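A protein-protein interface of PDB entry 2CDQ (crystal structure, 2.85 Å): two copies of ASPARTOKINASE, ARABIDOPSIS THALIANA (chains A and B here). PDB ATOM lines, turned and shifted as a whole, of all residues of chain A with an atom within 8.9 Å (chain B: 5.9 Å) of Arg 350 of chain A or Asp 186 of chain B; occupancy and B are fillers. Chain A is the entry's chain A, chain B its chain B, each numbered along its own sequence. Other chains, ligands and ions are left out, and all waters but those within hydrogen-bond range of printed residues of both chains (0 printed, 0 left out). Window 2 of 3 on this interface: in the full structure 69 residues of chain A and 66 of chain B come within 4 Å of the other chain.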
ATOM      1  N   ALA A 347      14.102  14.080   5.785  1.00  0.00           N
ATOM      2  CA  ALA A 347      14.886  13.792   6.995  1.00  0.00           C
ATOM      3  C   ALA A 347      14.762  14.849   8.080  1.00  0.00           C
ATOM      4  O   ALA A 347      14.923  16.037   7.815  1.00  0.00           O
ATOM      5  CB  ALA A 347      16.353  13.576   6.646  1.00  0.00           C
ATOM      6  N   SER A 348      14.484  14.403   9.303  1.00  0.00           N
ATOM      7  CA  SER A 348      14.464  15.283  10.472  1.00  0.00           C
ATOM      8  C   SER A 348      14.816  14.517  11.745  1.00  0.00           C
ATOM      9  O   SER A 348      14.331  13.410  11.955  1.00  0.00           O
ATOM     10  CB  SER A 348      13.094  15.958  10.626  1.00  0.00           C
ATOM     11  OG  SER A 348      13.038  16.754  11.802  1.00  0.00           O
ATOM     12  N   THR A 349      15.650  15.113  12.596  1.00  0.00           N
ATOM     13  CA  THR A 349      16.020  14.501  13.880  1.00  0.00           C
ATOM     14  C   THR A 349      14.846  14.506  14.873  1.00  0.00           C
ATOM     15  O   THR A 349      14.833  13.738  15.838  1.00  0.00           O
ATOM     16  CB  THR A 349      17.249  15.206  14.529  1.00  0.00           C
ATOM     17  OG1 THR A 349      16.921  16.564  14.855  1.00  0.00           O
ATOM     18  CG2 THR A 349      18.465  15.177  13.596  1.00  0.00           C
ATOM     19  N   ARG A 350      13.864  15.369  14.608  1.00  0.00           N
ATOM     20  CA  ARG A 350      12.728  15.598  15.502  1.00  0.00           C
ATOM     21  C   ARG A 350      11.647  14.521  15.457  1.00  0.00           C
ATOM     22  O   ARG A 350      10.870  14.391  16.404  1.00  0.00           O
ATOM     23  CB  ARG A 350      12.071  16.947  15.197  1.00  0.00           C
ATOM     24  CG  ARG A 350      12.887  18.170  15.572  1.00  0.00           C
ATOM     25  CD  ARG A 350      11.992  19.395  15.556  1.00  0.00           C
ATOM     26  NE  ARG A 350      12.740  20.622  15.291  1.00  0.00           N
ATOM     27  CZ  ARG A 350      13.342  21.356  16.223  1.00  0.00           C
ATOM     28  NH1 ARG A 350      13.299  20.990  17.500  1.00  0.00           N
ATOM     29  NH2 ARG A 350      13.991  22.460  15.875  1.00  0.00           N
ATOM     30  N   MET A 351      11.584  13.764  14.363  1.00  0.00           N
ATOM     31  CA  MET A 351      10.525  12.763  14.197  1.00  0.00           C
ATOM     32  C   MET A 351      10.680  11.530  15.098  1.00  0.00           C
ATOM     33  O   MET A 351       9.698  10.849  15.384  1.00  0.00           O
ATOM     34  CB  MET A 351      10.362  12.360  12.723  1.00  0.00           C
ATOM     35  CG  MET A 351      11.532  11.596  12.120  1.00  0.00           C
ATOM     36  SD  MET A 351      11.171  10.967  10.472  1.00  0.00           S
ATOM     37  CE  MET A 351      11.193  12.471   9.498  1.00  0.00           C
ATOM     38  N   LEU A 352      11.905  11.252  15.543  1.00  0.00           N
ATOM     39  CA  LEU A 352      12.161  10.109  16.418  1.00  0.00           C
ATOM     40  C   LEU A 352      11.561  10.363  17.801  1.00  0.00           C
ATOM     41  O   LEU A 352      12.129  11.092  18.619  1.00  0.00           O
ATOM     42  CB  LEU A 352      13.667   9.813  16.513  1.00  0.00           C
ATOM     43  CG  LEU A 352      14.129   8.412  16.953  1.00  0.00           C
ATOM     44  CD1 LEU A 352      15.640   8.304  16.872  1.00  0.00           C
ATOM     45  CD2 LEU A 352      13.658   8.033  18.352  1.00  0.00           C
ATOM     46  N   GLY A 353      10.404   9.759  18.049  1.00  0.00           N
ATOM     47  CA  GLY A 353       9.685   9.945  19.305  1.00  0.00           C
ATOM     48  C   GLY A 353       8.635  11.048  19.299  1.00  0.00           C
ATOM     49  O   GLY A 353       8.125  11.419  20.361  1.00  0.00           O
ATOM     50  N   GLN A 354       8.309  11.579  18.120  1.00  0.00           N
ATOM     51  CA  GLN A 354       7.285  12.615  18.007  1.00  0.00           C
ATOM     52  C   GLN A 354       5.983  12.065  17.454  1.00  0.00           C
ATOM     53  O   GLN A 354       5.988  11.285  16.510  1.00  0.00           O
ATOM     54  CB  GLN A 354       7.761  13.767  17.112  1.00  0.00           C
ATOM     55  CG  GLN A 354       6.806  14.967  17.126  1.00  0.00           C
ATOM     56  CD  GLN A 354       7.286  16.126  16.274  1.00  0.00           C
ATOM     57  OE1 GLN A 354       6.984  16.208  15.081  1.00  0.00           O
ATOM     58  NE2 GLN A 354       8.023  17.044  16.891  1.00  0.00           N
ATOM     59  N   VAL A 355       4.871  12.477  18.050  1.00  0.00           N
ATOM     60  CA  VAL A 355       3.543  12.177  17.515  1.00  0.00           C
ATOM     61  C   VAL A 355       3.239  13.198  16.418  1.00  0.00           C
ATOM     62  O   VAL A 355       3.431  14.398  16.612  1.00  0.00           O
ATOM     63  CB  VAL A 355       2.438  12.239  18.621  1.00  0.00           C
ATOM     64  CG1 VAL A 355       1.059  11.989  18.035  1.00  0.00           C
ATOM     65  CG2 VAL A 355       2.715  11.238  19.734  1.00  0.00           C
ATOM     66  N   GLY A 356       2.803  12.717  15.254  1.00  0.00           N
ATOM     67  CA  GLY A 356       2.245  13.610  14.222  1.00  0.00           C
ATOM     68  C   GLY A 356       3.150  14.118  13.106  1.00  0.00           C
ATOM     69  O   GLY A 356       2.744  15.004  12.350  1.00  0.00           O
ATOM     70  N   PHE A 357       4.365  13.584  12.988  1.00  0.00           N
ATOM     71  CA  PHE A 357       5.241  13.949  11.864  1.00  0.00           C
ATOM     72  C   PHE A 357       4.764  13.289  10.573  1.00  0.00           C
ATOM     73  O   PHE A 357       4.718  13.936   9.523  1.00  0.00           O
ATOM     74  CB  PHE A 357       6.713  13.609  12.128  1.00  0.00           C
ATOM     75  CG  PHE A 357       7.669  14.460  11.352  1.00  0.00           C
ATOM     76  CD1 PHE A 357       8.291  15.553  11.955  1.00  0.00           C
ATOM     77  CD2 PHE A 357       7.939  14.191  10.012  1.00  0.00           C
ATOM     78  CE1 PHE A 357       9.176  16.360  11.239  1.00  0.00           C
ATOM     79  CE2 PHE A 357       8.816  14.992   9.286  1.00  0.00           C
ATOM     80  CZ  PHE A 357       9.441  16.080   9.903  1.00  0.00           C
ATOM     81  N   GLU A 379      15.303   5.835  11.243  1.00  0.00           N
ATOM     82  CA  GLU A 379      15.089   6.434  12.572  1.00  0.00           C
ATOM     83  C   GLU A 379      14.806   7.934  12.517  1.00  0.00           C
ATOM     84  O   GLU A 379      14.081   8.455  13.360  1.00  0.00           O
ATOM     85  CB  GLU A 379      16.267   6.165  13.522  1.00  0.00           C
ATOM     86  CG  GLU A 379      16.702   4.699  13.639  1.00  0.00           C
ATOM     87  CD  GLU A 379      15.684   3.803  14.331  1.00  0.00           C
ATOM     88  OE1 GLU A 379      14.755   4.315  14.996  1.00  0.00           O
ATOM     89  OE2 GLU A 379      15.823   2.567  14.207  1.00  0.00           O
ATOM     90  N   VAL A 380      15.377   8.617  11.526  1.00  0.00           N
ATOM     91  CA  VAL A 380      15.212  10.074  11.385  1.00  0.00           C
ATOM     92  C   VAL A 380      14.827  10.522   9.974  1.00  0.00           C
ATOM     93  O   VAL A 380      15.064  11.674   9.591  1.00  0.00           O
ATOM     94  CB  VAL A 380      16.485  10.855  11.818  1.00  0.00           C
ATOM     95  CG1 VAL A 380      16.723  10.704  13.301  1.00  0.00           C
ATOM     96  CG2 VAL A 380      17.705  10.413  11.009  1.00  0.00           C
ATOM     97  N   SER A 381      14.246   9.618   9.197  1.00  0.00           N
ATOM     98  CA  SER A 381      13.840   9.960   7.843  1.00  0.00           C
ATOM     99  C   SER A 381      12.671   9.128   7.367  1.00  0.00           C
ATOM    100  O   SER A 381      12.471   7.989   7.809  1.00  0.00           O
ATOM    101  CB  SER A 381      15.008   9.826   6.858  1.00  0.00           C
ATOM    102  OG  SER A 381      15.283   8.469   6.544  1.00  0.00           O
ATOM    103  N   LYS A 410       9.779  23.175   5.189  1.00  0.00           N
ATOM    104  CA  LYS A 410       9.417  23.921   6.397  1.00  0.00           C
ATOM    105  C   LYS A 410       9.565  23.062   7.648  1.00  0.00           C
ATOM    106  O   LYS A 410       9.790  23.590   8.738  1.00  0.00           O
ATOM    107  CB  LYS A 410       7.978  24.437   6.314  1.00  0.00           C
ATOM    108  CG  LYS A 410       7.708  25.416   5.186  1.00  0.00           C
ATOM    109  CD  LYS A 410       6.269  25.913   5.242  1.00  0.00           C
ATOM    110  CE  LYS A 410       5.964  26.897   4.113  1.00  0.00           C
ATOM    111  NZ  LYS A 410       4.621  27.526   4.274  1.00  0.00           N
ATOM    112  N   ILE A 411       9.433  21.743   7.497  1.00  0.00           N
ATOM    113  CA  ILE A 411       9.522  20.828   8.644  1.00  0.00           C
ATOM    114  C   ILE A 411      10.704  19.859   8.602  1.00  0.00           C
ATOM    115  O   ILE A 411      11.003  19.216   9.613  1.00  0.00           O
ATOM    116  CB  ILE A 411       8.209  20.027   8.876  1.00  0.00           C
ATOM    117  CG1 ILE A 411       7.795  19.279   7.605  1.00  0.00           C
ATOM    118  CG2 ILE A 411       7.098  20.944   9.389  1.00  0.00           C
ATOM    119  CD1 ILE A 411       6.768  18.185   7.847  1.00  0.00           C
ATOM    120  N   ALA A 412      11.370  19.758   7.448  1.00  0.00           N
ATOM    121  CA  ALA A 412      12.478  18.804   7.273  1.00  0.00           C
ATOM    122  C   ALA A 412      13.524  19.207   6.223  1.00  0.00           C
ATOM    123  O   ALA A 412      13.377  20.227   5.540  1.00  0.00           O
ATOM    124  CB  ALA A 412      11.931  17.417   6.957  1.00  0.00           C
ATOM    125  N   ILE B 177      18.445  29.015  27.508  1.00  0.00           N
ATOM    126  CA  ILE B 177      17.139  29.602  27.196  1.00  0.00           C
ATOM    127  C   ILE B 177      16.402  28.728  26.183  1.00  0.00           C
ATOM    128  O   ILE B 177      16.924  28.445  25.099  1.00  0.00           O
ATOM    129  CB  ILE B 177      17.273  31.066  26.653  1.00  0.00           C
ATOM    130  CG1 ILE B 177      18.309  31.885  27.452  1.00  0.00           C
ATOM    131  CG2 ILE B 177      15.908  31.765  26.604  1.00  0.00           C
ATOM    132  CD1 ILE B 177      18.003  32.083  28.960  1.00  0.00           C
ATOM    133  N   THR B 178      15.194  28.299  26.544  1.00  0.00           N
ATOM    134  CA  THR B 178      14.402  27.405  25.691  1.00  0.00           C
ATOM    135  C   THR B 178      13.020  27.972  25.378  1.00  0.00           C
ATOM    136  O   THR B 178      12.689  29.085  25.790  1.00  0.00           O
ATOM    137  CB  THR B 178      14.195  26.026  26.346  1.00  0.00           C
ATOM    138  OG1 THR B 178      13.324  26.159  27.476  1.00  0.00           O
ATOM    139  CG2 THR B 178      15.523  25.412  26.779  1.00  0.00           C
ATOM    140  N   THR B 179      12.217  27.198  24.646  1.00  0.00           N
ATOM    141  CA  THR B 179      10.804  27.525  24.441  1.00  0.00           C
ATOM    142  C   THR B 179      10.039  27.150  25.704  1.00  0.00           C
ATOM    143  O   THR B 179      10.626  26.643  26.662  1.00  0.00           O
ATOM    144  CB  THR B 179      10.192  26.804  23.212  1.00  0.00           C
ATOM    145  OG1 THR B 179      10.199  25.389  23.424  1.00  0.00           O
ATOM    146  CG2 THR B 179      10.954  27.141  21.935  1.00  0.00           C
ATOM    147  N   ASP B 181       7.284  25.022  26.027  1.00  0.00           N
ATOM    148  CA  ASP B 181       6.573  23.742  26.104  1.00  0.00           C
ATOM    149  C   ASP B 181       7.450  22.746  26.848  1.00  0.00           C
ATOM    150  O   ASP B 181       8.631  22.578  26.535  1.00  0.00           O
ATOM    151  CB  ASP B 181       6.091  23.227  24.736  1.00  0.00           C
ATOM    152  CG  ASP B 181       7.165  23.278  23.669  1.00  0.00           C
ATOM    153  OD1 ASP B 181       7.428  22.216  23.064  1.00  0.00           O
ATOM    154  OD2 ASP B 181       7.733  24.369  23.428  1.00  0.00           O
ATOM    155  N   ASN B 184       9.289  19.020  26.504  1.00  0.00           N
ATOM    156  CA  ASN B 184      10.115  19.150  25.307  1.00  0.00           C
ATOM    157  C   ASN B 184      10.587  20.593  25.049  1.00  0.00           C
ATOM    158  O   ASN B 184      10.147  21.248  24.104  1.00  0.00           O
ATOM    159  CB  ASN B 184       9.337  18.593  24.102  1.00  0.00           C
ATOM    160  CG  ASN B 184      10.163  18.546  22.830  1.00  0.00           C
ATOM    161  OD1 ASN B 184      11.391  18.413  22.866  1.00  0.00           O
ATOM    162  ND2 ASN B 184       9.484  18.650  21.689  1.00  0.00           N
ATOM    163  N   GLY B 185      11.488  21.083  25.895  1.00  0.00           N
ATOM    164  CA  GLY B 185      12.030  22.437  25.752  1.00  0.00           C
ATOM    165  C   GLY B 185      13.049  22.571  24.636  1.00  0.00           C
ATOM    166  O   GLY B 185      14.096  21.921  24.649  1.00  0.00           O
ATOM    167  N   ASP B 186      12.744  23.424  23.668  1.00  0.00           N
ATOM    168  CA  ASP B 186      13.605  23.602  22.509  1.00  0.00           C
ATOM    169  C   ASP B 186      14.619  24.722  22.748  1.00  0.00           C
ATOM    170  O   ASP B 186      14.242  25.876  22.964  1.00  0.00           O
ATOM    171  CB  ASP B 186      12.752  23.899  21.272  1.00  0.00           C
ATOM    172  CG  ASP B 186      13.484  23.631  19.965  1.00  0.00           C
ATOM    173  OD1 ASP B 186      14.617  23.105  19.991  1.00  0.00           O
ATOM    174  OD2 ASP B 186      12.914  23.945  18.900  1.00  0.00           O
ATOM    175  N   ILE B 187      15.904  24.375  22.710  1.00  0.00           N
ATOM    176  CA  ILE B 187      16.974  25.355  22.909  1.00  0.00           C
ATOM    177  C   ILE B 187      16.945  26.464  21.850  1.00  0.00           C
ATOM    178  O   ILE B 187      16.964  26.186  20.647  1.00  0.00           O
ATOM    179  CB  ILE B 187      18.371  24.691  22.926  1.00  0.00           C
ATOM    180  CG1 ILE B 187      18.470  23.686  24.082  1.00  0.00           C
ATOM    181  CG2 ILE B 187      19.469  25.758  23.009  1.00  0.00           C
ATOM    182  CD1 ILE B 187      19.867  23.139  24.336  1.00  0.00           C
ATOM    183  N   LEU B 188      16.899  27.714  22.314  1.00  0.00           N
ATOM    184  CA  LEU B 188      16.871  28.889  21.436  1.00  0.00           C
ATOM    185  C   LEU B 188      18.259  29.476  21.192  1.00  0.00           C
ATOM    186  O   LEU B 188      19.112  29.448  22.080  1.00  0.00           O
ATOM    187  CB  LEU B 188      15.934  29.958  22.000  1.00  0.00           C
ATOM    188  CG  LEU B 188      14.454  29.576  22.080  1.00  0.00           C
ATOM    189  CD1 LEU B 188      13.675  30.691  22.754  1.00  0.00           C
ATOM    190  CD2 LEU B 188      13.881  29.270  20.692  1.00  0.00           C
ATOM    191  N   THR B 226      12.673  24.149  32.746  1.00  0.00           N
ATOM    192  CA  THR B 226      12.343  23.348  31.578  1.00  0.00           C
ATOM    193  C   THR B 226      13.307  22.171  31.407  1.00  0.00           C
ATOM    194  O   THR B 226      14.495  22.290  31.706  1.00  0.00           O
ATOM    195  CB  THR B 226      12.318  24.249  30.322  1.00  0.00           C
ATOM    196  OG1 THR B 226      10.981  24.718  30.113  1.00  0.00           O
ATOM    197  CG2 THR B 226      12.778  23.513  29.084  1.00  0.00           C
ATOM    198  N   THR B 227      12.786  21.036  30.942  1.00  0.00           N
ATOM    199  CA  THR B 227      13.634  19.909  30.556  1.00  0.00           C
ATOM    200  C   THR B 227      13.798  19.854  29.045  1.00  0.00           C
ATOM    201  O   THR B 227      12.880  20.189  28.302  1.00  0.00           O
ATOM    202  CB  THR B 227      13.118  18.556  31.084  1.00  0.00           C
ATOM    203  OG1 THR B 227      11.787  18.332  30.624  1.00  0.00           O
ATOM    204  CG2 THR B 227      13.132  18.537  32.585  1.00  0.00           C
ATOM    205  N   LEU B 228      14.971  19.413  28.596  1.00  0.00           N
ATOM    206  CA  LEU B 228      15.345  19.507  27.184  1.00  0.00           C
ATOM    207  C   LEU B 228      14.758  18.428  26.261  1.00  0.00           C
ATOM    208  O   LEU B 228      15.111  18.363  25.084  1.00  0.00           O
ATOM    209  CB  LEU B 228      16.871  19.566  27.051  1.00  0.00           C
ATOM    210  CG  LEU B 228      17.584  20.668  27.847  1.00  0.00           C
ATOM    211  CD1 LEU B 228      19.092  20.559  27.681  1.00  0.00           C
ATOM    212  CD2 LEU B 228      17.105  22.057  27.459  1.00  0.00           C
ATOM    213  N   HIS B 292      20.803  10.857  21.355  1.00  0.00           N
ATOM    214  CA  HIS B 292      19.596  10.967  20.550  1.00  0.00           C
ATOM    215  C   HIS B 292      19.909  11.947  19.426  1.00  0.00           C
ATOM    216  O   HIS B 292      20.609  12.936  19.657  1.00  0.00           O
ATOM    217  CB  HIS B 292      18.436  11.475  21.401  1.00  0.00           C
ATOM    218  CG  HIS B 292      17.169  11.699  20.635  1.00  0.00           C
ATOM    219  ND1 HIS B 292      16.972  12.798  19.825  1.00  0.00           N
ATOM    220  CD2 HIS B 292      16.031  10.970  20.563  1.00  0.00           C
ATOM    221  CE1 HIS B 292      15.770  12.734  19.283  1.00  0.00           C
ATOM    222  NE2 HIS B 292      15.177  11.636  19.716  1.00  0.00           N
ATOM    223  N   GLN B 294      18.761  14.407  18.057  1.00  0.00           N
ATOM    224  CA  GLN B 294      18.551  15.819  18.341  1.00  0.00           C
ATOM    225  C   GLN B 294      19.698  16.434  19.146  1.00  0.00           C
ATOM    226  O   GLN B 294      19.979  17.626  19.024  1.00  0.00           O
ATOM    227  CB  GLN B 294      17.236  15.989  19.087  1.00  0.00           C
ATOM    228  CG  GLN B 294      16.634  17.364  19.001  1.00  0.00           C
ATOM    229  CD  GLN B 294      15.329  17.442  19.754  1.00  0.00           C
ATOM    230  OE1 GLN B 294      14.256  17.480  19.150  1.00  0.00           O
ATOM    231  NE2 GLN B 294      15.407  17.437  21.087  1.00  0.00           N
ATOM    232  N   ARG B 297      22.982  17.770  17.009  1.00  0.00           N
ATOM    233  CA  ARG B 297      22.863  18.908  16.096  1.00  0.00           C
ATOM    234  C   ARG B 297      23.816  20.077  16.394  1.00  0.00           C
ATOM    235  O   ARG B 297      24.446  20.589  15.463  1.00  0.00           O
ATOM    236  CB  ARG B 297      21.415  19.380  15.981  1.00  0.00           C
ATOM    237  CG  ARG B 297      20.600  18.607  14.958  1.00  0.00           C
ATOM    238  CD  ARG B 297      19.273  19.295  14.723  1.00  0.00           C
ATOM    239  NE  ARG B 297      18.536  19.457  15.975  1.00  0.00           N
ATOM    240  CZ  ARG B 297      17.497  20.272  16.147  1.00  0.00           C
ATOM    241  NH1 ARG B 297      17.048  21.022  15.145  1.00  0.00           N
ATOM    242  NH2 ARG B 297      16.904  20.338  17.334  1.00  0.00           N
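O of Thr 349 of chain A touches CE1 of His 292 of chain B (3.7 Å).
Thr 349 of chain A touches Gln 294 of chain B.
Arg 350 of chain A touches Gln 294 of chain B (CG to OE1, 3.9 Å).
The backbone NH (N) of Arg 350 of chain A sits close to the side-chain hydroxyl (OG) of Ser 348 of chain A, at 3.2 Å.
The backbone NH of Thr 179 of chain B is in hydrogen-bond range of the backbone carbonyl oxygen of Asp 186 of chain B, 2.9 Å away.
A ring nitrogen (ND1) of His 292 of chain B sits at hydrogen-bond distance from the backbone NH (N) of Gln 294 of chain B (3.0 Å).
No position is printed for both chains.
Hydrophobic or aromatic side chains of chain A that line the printed part of chain B: Leu 352.
Hydrophobic or aromatic side chains of chain B that line the printed part of chain A: His 292.
Along chain B the printed residues that touch a printed residue of chain A span positions 186 to 297.
Among the printed residues, 7 pairs touch across the chains.
Among the printed residues, Asp or Glu carboxylates within 4 Å of a Lys or Arg side-chain nitrogen of the other chain: Arg 350 of chain A with Asp 186 of chain B (3.3 Å).
NH1 of Arg 297 of chain B lies close to NH2 of Arg 350 of chain A (3.5 Å).
A ring nitrogen (NE2) of His 292 of chain B is in hydrogen-bond range of the backbone carbonyl oxygen (O) of Leu 352 of chain A (3.3 Å).
OG1 of Thr 349 of chain A is in hydrogen-bond range of NE of Arg 297 of chain B (3.5 Å).
OD2 of Asp 186 of chain B lies within salt-bridge range of NH1 of Arg 350 of chain A, at 3.3 Å.
Of chain B, only Asp 186, Gln 294 and Arg 297 come within 4 Å of Arg 350 of chain A.
Of the printed residues of chain A, Asp 186 of chain B touches Arg 350 (3.3 Å).
Of the printed residues of chain A, Arg 297 of chain B touches Thr 349 and Arg 350.
Printed residues of chain B within 4 Å of Thr 349 of chain A: His 292 (3.7 Å), Gln 294 (3.9 Å) and Arg 297 (3.5 Å).
Printed residues of chain B within 4 Å of Leu 352 of chain A: His 292.
Printed residues of chain A within 4 Å of Gln 294 of chain B: Thr 349 (3.9 Å) and Arg 350 (3.9 Å).
Of the printed residues of chain A, His 292 of chain B touches Thr 349 (3.7 Å) and Leu 352 (3.3 Å).
Ile 411 of chain A touches none of the printed residues of chain B.
Lys 410 of chain A touches none of the printed residues of chain B.
The nearest residue of chain B that does not touch Arg 350 of chain A is His 292 of chain B (5.6 Å).
The nearest residue of chain A that does not touch Asp 186 of chain B is Thr 349 of chain A (8.6 Å).
The nearest printed residue of chain A that does not touch Arg 297 of chain B is Ser 348 of chain A (6.7 Å).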
